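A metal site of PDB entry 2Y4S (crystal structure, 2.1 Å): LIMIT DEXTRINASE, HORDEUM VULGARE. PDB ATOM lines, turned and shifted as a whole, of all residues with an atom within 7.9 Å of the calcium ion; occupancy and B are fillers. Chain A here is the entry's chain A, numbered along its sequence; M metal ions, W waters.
ND2 of Asn 700 sits at hydrogen-bond distance from OE2 of Glu 348 (3.2 Å).
Of the 18 residues printed, 4 come within 4 Å of the calcium ion.
O of Tyr 352 is bound to the calcium ion. The backbone carbonyl oxygen (O) of Gln 347 is bound to the calcium ion, at 2.4 Å. The calcium ion is bound by OD1 of Asn 700, at 2.6 Å. The calcium ion is bound by the side-chain carboxylate (OD1) of Asp 350, 2.6 Å away. Water W2 is bound to the calcium ion (2.7 Å). The calcium ion is bound by water W1, at 2.7 Å. The calcium ion is bound by water W3 (2.8 Å). The calcium ion has seven donor atoms within binding distance.
Water W2 bridges the backbone carbonyl oxygen (O) of Gly 313 (2.6 Å) and the side-chain amide nitrogen (ND2) of Asn 353 (2.8 Å). Water W3 lies within hydrogen-bond range of OD2 of Asp 350 (2.6 Å), O of Asn 700 (2.8 Å) and N of Gly 702 (3.1 Å). Water W1 bridges O of Asp 350 (2.5 Å) and O of Gly 313 (2.7 Å).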
ATOM      1  N   GLY A 313     -18.971  15.985 -15.110  1.00  0.00           N
ATOM      2  CA  GLY A 313     -19.418  15.451 -13.832  1.00  0.00           C
ATOM      3  C   GLY A 313     -20.905  15.580 -13.617  1.00  0.00           C
ATOM      4  O   GLY A 313     -21.461  14.979 -12.702  1.00  0.00           O
ATOM      5  N   VAL A 314     -21.553  16.366 -14.465  1.00  0.00           N
ATOM      6  CA  VAL A 314     -23.009  16.535 -14.428  1.00  0.00           C
ATOM      7  C   VAL A 314     -23.556  16.531 -15.849  1.00  0.00           C
ATOM      8  O   VAL A 314     -23.087  17.283 -16.712  1.00  0.00           O
ATOM      9  CB  VAL A 314     -23.418  17.868 -13.756  1.00  0.00           C
ATOM     10  CG1 VAL A 314     -24.927  18.037 -13.810  1.00  0.00           C
ATOM     11  CG2 VAL A 314     -22.920  17.922 -12.309  1.00  0.00           C
ATOM     12  N   ASP A 315     -24.536  15.672 -16.109  1.00  0.00           N
ATOM     13  CA  ASP A 315     -25.167  15.605 -17.422  1.00  0.00           C
ATOM     14  C   ASP A 315     -25.995  16.865 -17.652  1.00  0.00           C
ATOM     15  O   ASP A 315     -26.775  17.273 -16.772  1.00  0.00           O
ATOM     16  CB  ASP A 315     -26.042  14.352 -17.503  1.00  0.00           C
ATOM     17  CG  ASP A 315     -26.377  13.953 -18.925  1.00  0.00           C
ATOM     18  OD1 ASP A 315     -26.592  14.840 -19.769  1.00  0.00           O
ATOM     19  OD2 ASP A 315     -26.427  12.729 -19.198  1.00  0.00           O
ATOM     20  N   VAL A 343     -26.901   8.562  -1.284  1.00  0.00           N
ATOM     21  CA  VAL A 343     -26.314   9.592  -2.144  1.00  0.00           C
ATOM     22  C   VAL A 343     -25.181   9.021  -2.992  1.00  0.00           C
ATOM     23  O   VAL A 343     -25.145   9.209  -4.211  1.00  0.00           O
ATOM     24  CB  VAL A 343     -25.797  10.786  -1.316  1.00  0.00           C
ATOM     25  CG1 VAL A 343     -25.091  11.795  -2.221  1.00  0.00           C
ATOM     26  CG2 VAL A 343     -26.944  11.448  -0.569  1.00  0.00           C
ATOM     27  N   ILE A 346     -25.889   7.120  -6.243  1.00  0.00           N
ATOM     28  CA  ILE A 346     -26.301   7.815  -7.467  1.00  0.00           C
ATOM     29  C   ILE A 346     -25.447   9.031  -7.795  1.00  0.00           C
ATOM     30  O   ILE A 346     -25.705   9.740  -8.767  1.00  0.00           O
ATOM     31  CB  ILE A 346     -27.778   8.292  -7.384  1.00  0.00           C
ATOM     32  CG1 ILE A 346     -27.928   9.356  -6.299  1.00  0.00           C
ATOM     33  CG2 ILE A 346     -28.720   7.116  -7.145  1.00  0.00           C
ATOM     34  CD1 ILE A 346     -29.227  10.115  -6.362  1.00  0.00           C
ATOM     35  N   GLN A 347     -24.426   9.280  -6.977  1.00  0.00           N
ATOM     36  CA  GLN A 347     -23.666  10.515  -7.076  1.00  0.00           C
ATOM     37  C   GLN A 347     -23.011  10.741  -8.438  1.00  0.00           C
ATOM     38  O   GLN A 347     -22.671  11.855  -8.769  1.00  0.00           O
ATOM     39  CB  GLN A 347     -22.616  10.621  -5.960  1.00  0.00           C
ATOM     40  CG  GLN A 347     -21.385   9.754  -6.198  1.00  0.00           C
ATOM     41  CD  GLN A 347     -20.438   9.760  -5.008  1.00  0.00           C
ATOM     42  OE1 GLN A 347     -20.449  10.677  -4.188  1.00  0.00           O
ATOM     43  NE2 GLN A 347     -19.595   8.743  -4.930  1.00  0.00           N
ATOM     44  N   GLU A 348     -22.819   9.687  -9.214  1.00  0.00           N
ATOM     45  CA  GLU A 348     -22.173   9.854 -10.511  1.00  0.00           C
ATOM     46  C   GLU A 348     -23.154  10.303 -11.596  1.00  0.00           C
ATOM     47  O   GLU A 348     -22.748  10.711 -12.684  1.00  0.00           O
ATOM     48  CB  GLU A 348     -21.442   8.582 -10.948  1.00  0.00           C
ATOM     49  CG  GLU A 348     -20.262   8.219 -10.058  1.00  0.00           C
ATOM     50  CD  GLU A 348     -19.207   9.307 -10.020  1.00  0.00           C
ATOM     51  OE1 GLU A 348     -18.862   9.840 -11.091  1.00  0.00           O
ATOM     52  OE2 GLU A 348     -18.710   9.624  -8.922  1.00  0.00           O
ATOM     53  N   GLU A 349     -24.443  10.219 -11.300  1.00  0.00           N
ATOM     54  CA  GLU A 349     -25.473  10.552 -12.286  1.00  0.00           C
ATOM     55  C   GLU A 349     -26.539  11.498 -11.752  1.00  0.00           C
ATOM     56  O   GLU A 349     -27.621  11.591 -12.320  1.00  0.00           O
ATOM     57  CB  GLU A 349     -26.135   9.272 -12.814  1.00  0.00           C
ATOM     58  CG  GLU A 349     -25.193   8.292 -13.491  1.00  0.00           C
ATOM     59  CD  GLU A 349     -24.706   7.212 -12.543  1.00  0.00           C
ATOM     60  OE1 GLU A 349     -25.487   6.808 -11.647  1.00  0.00           O
ATOM     61  OE2 GLU A 349     -23.559   6.746 -12.697  1.00  0.00           O
ATOM     62  N   ASP A 350     -26.239  12.190 -10.650  1.00  0.00           N
ATOM     63  CA  ASP A 350     -27.189  13.166 -10.109  1.00  0.00           C
ATOM     64  C   ASP A 350     -26.897  14.549 -10.686  1.00  0.00           C
ATOM     65  O   ASP A 350     -26.012  14.698 -11.527  1.00  0.00           O
ATOM     66  CB  ASP A 350     -27.193  13.138  -8.580  1.00  0.00           C
ATOM     67  CG  ASP A 350     -25.962  13.773  -7.975  1.00  0.00           C
ATOM     68  OD1 ASP A 350     -25.137  14.298  -8.745  1.00  0.00           O
ATOM     69  OD2 ASP A 350     -25.834  13.760  -6.739  1.00  0.00           O
ATOM     70  N   PRO A 351     -27.649  15.584 -10.248  1.00  0.00           N
ATOM     71  CA  PRO A 351     -27.447  16.886 -10.882  1.00  0.00           C
ATOM     72  C   PRO A 351     -26.309  17.707 -10.266  1.00  0.00           C
ATOM     73  O   PRO A 351     -26.147  18.864 -10.653  1.00  0.00           O
ATOM     74  CB  PRO A 351     -28.776  17.615 -10.602  1.00  0.00           C
ATOM     75  CG  PRO A 351     -29.695  16.600  -9.949  1.00  0.00           C
ATOM     76  CD  PRO A 351     -28.788  15.596  -9.321  1.00  0.00           C
ATOM     77  N   TYR A 352     -25.546  17.124  -9.353  1.00  0.00           N
ATOM     78  CA  TYR A 352     -24.698  17.921  -8.470  1.00  0.00           C
ATOM     79  C   TYR A 352     -23.187  17.771  -8.640  1.00  0.00           C
ATOM     80  O   TYR A 352     -22.670  16.668  -8.717  1.00  0.00           O
ATOM     81  CB  TYR A 352     -25.042  17.627  -7.014  1.00  0.00           C
ATOM     82  CG  TYR A 352     -24.470  18.664  -6.074  1.00  0.00           C
ATOM     83  CD1 TYR A 352     -23.168  18.562  -5.608  1.00  0.00           C
ATOM     84  CD2 TYR A 352     -25.234  19.758  -5.688  1.00  0.00           C
ATOM     85  CE1 TYR A 352     -22.645  19.529  -4.755  1.00  0.00           C
ATOM     86  CE2 TYR A 352     -24.714  20.725  -4.849  1.00  0.00           C
ATOM     87  CZ  TYR A 352     -23.422  20.606  -4.382  1.00  0.00           C
ATOM     88  OH  TYR A 352     -22.926  21.574  -3.545  1.00  0.00           O
ATOM     89  N   ASN A 353     -22.478  18.892  -8.654  1.00  0.00           N
ATOM     90  CA  ASN A 353     -21.023  18.888  -8.583  1.00  0.00           C
ATOM     91  C   ASN A 353     -20.518  20.309  -8.400  1.00  0.00           C
ATOM     92  O   ASN A 353     -21.094  21.233  -8.968  1.00  0.00           O
ATOM     93  CB  ASN A 353     -20.410  18.249  -9.836  1.00  0.00           C
ATOM     94  CG  ASN A 353     -18.962  17.828  -9.629  1.00  0.00           C
ATOM     95  OD1 ASN A 353     -18.058  18.671  -9.528  1.00  0.00           O
ATOM     96  ND2 ASN A 353     -18.729  16.521  -9.565  1.00  0.00           N
ATOM     97  N   TRP A 354     -19.465  20.494  -7.613  1.00  0.00           N
ATOM     98  CA  TRP A 354     -18.911  21.841  -7.471  1.00  0.00           C
ATOM     99  C   TRP A 354     -18.561  22.386  -8.846  1.00  0.00           C
ATOM    100  O   TRP A 354     -18.781  23.560  -9.120  1.00  0.00           O
ATOM    101  CB  TRP A 354     -17.673  21.856  -6.577  1.00  0.00           C
ATOM    102  CG  TRP A 354     -17.960  21.782  -5.108  1.00  0.00           C
ATOM    103  CD1 TRP A 354     -19.161  21.989  -4.493  1.00  0.00           C
ATOM    104  CD2 TRP A 354     -17.018  21.521  -4.066  1.00  0.00           C
ATOM    105  NE1 TRP A 354     -19.023  21.854  -3.133  1.00  0.00           N
ATOM    106  CE2 TRP A 354     -17.724  21.562  -2.841  1.00  0.00           C
ATOM    107  CE3 TRP A 354     -15.648  21.231  -4.048  1.00  0.00           C
ATOM    108  CZ2 TRP A 354     -17.101  21.333  -1.618  1.00  0.00           C
ATOM    109  CZ3 TRP A 354     -15.033  21.006  -2.830  1.00  0.00           C
ATOM    110  CH2 TRP A 354     -15.756  21.054  -1.631  1.00  0.00           C
ATOM    111  N   TYR A 699     -17.884  18.097  -2.581  1.00  0.00           N
ATOM    112  CA  TYR A 699     -17.930  18.360  -4.018  1.00  0.00           C
ATOM    113  C   TYR A 699     -18.882  17.443  -4.784  1.00  0.00           C
ATOM    114  O   TYR A 699     -19.406  17.812  -5.833  1.00  0.00           O
ATOM    115  CB  TYR A 699     -16.519  18.247  -4.621  1.00  0.00           C
ATOM    116  CG  TYR A 699     -16.050  16.821  -4.825  1.00  0.00           C
ATOM    117  CD1 TYR A 699     -15.611  16.045  -3.762  1.00  0.00           C
ATOM    118  CD2 TYR A 699     -16.047  16.242  -6.098  1.00  0.00           C
ATOM    119  CE1 TYR A 699     -15.189  14.736  -3.951  1.00  0.00           C
ATOM    120  CE2 TYR A 699     -15.611  14.948  -6.297  1.00  0.00           C
ATOM    121  CZ  TYR A 699     -15.190  14.193  -5.215  1.00  0.00           C
ATOM    122  OH  TYR A 699     -14.766  12.905  -5.412  1.00  0.00           O
ATOM    123  N   ASN A 700     -19.089  16.238  -4.260  1.00  0.00           N
ATOM    124  CA  ASN A 700     -19.894  15.227  -4.943  1.00  0.00           C
ATOM    125  C   ASN A 700     -20.957  14.668  -4.019  1.00  0.00           C
ATOM    126  O   ASN A 700     -21.463  13.562  -4.232  1.00  0.00           O
ATOM    127  CB  ASN A 700     -18.983  14.105  -5.453  1.00  0.00           C
ATOM    128  CG  ASN A 700     -19.543  13.406  -6.677  1.00  0.00           C
ATOM    129  OD1 ASN A 700     -20.428  13.921  -7.345  1.00  0.00           O
ATOM    130  ND2 ASN A 700     -19.015  12.225  -6.998  1.00  0.00           N
ATOM    131  N   SER A 701     -21.289  15.428  -2.976  1.00  0.00           N
ATOM    132  CA  SER A 701     -22.180  14.967  -1.916  1.00  0.00           C
ATOM    133  C   SER A 701     -23.653  15.309  -2.157  1.00  0.00           C
ATOM    134  O   SER A 701     -24.483  15.146  -1.256  1.00  0.00           O
ATOM    135  CB  SER A 701     -21.723  15.513  -0.562  1.00  0.00           C
ATOM    136  OG  SER A 701     -20.445  14.997  -0.225  1.00  0.00           O
ATOM    137  N   GLY A 702     -23.960  15.781  -3.360  1.00  0.00           N
ATOM    138  CA  GLY A 702     -25.343  15.996  -3.769  1.00  0.00           C
ATOM    139  C   GLY A 702     -26.058  17.110  -3.024  1.00  0.00           C
ATOM    140  O   GLY A 702     -25.490  17.781  -2.171  1.00  0.00           O
ATOM    141  N   ASP A 703     -27.325  17.314  -3.362  1.00  0.00           N
ATOM    142  CA  ASP A 703     -28.135  18.336  -2.711  1.00  0.00           C
ATOM    143  C   ASP A 703     -28.349  18.032  -1.238  1.00  0.00           C
ATOM    144  O   ASP A 703     -28.564  18.942  -0.435  1.00  0.00           O
ATOM    145  CB  ASP A 703     -29.489  18.484  -3.416  1.00  0.00           C
ATOM    146  CG  ASP A 703     -29.365  19.080  -4.794  1.00  0.00           C
ATOM    147  OD1 ASP A 703     -28.486  19.940  -4.990  1.00  0.00           O
ATOM    148  OD2 ASP A 703     -30.149  18.691  -5.679  1.00  0.00           O
HETATM  149 CA    CA M   1     -22.558  14.278  -8.703  1.00  0.00          CA
HETATM  150  O   HOH W   1     -23.547  14.209 -11.259  1.00  0.00           O
HETATM  151  O   HOH W   2     -20.471  14.423 -10.353  1.00  0.00           O
HETATM  152  O   HOH W   3     -23.396  14.432  -6.062  1.00  0.00           O
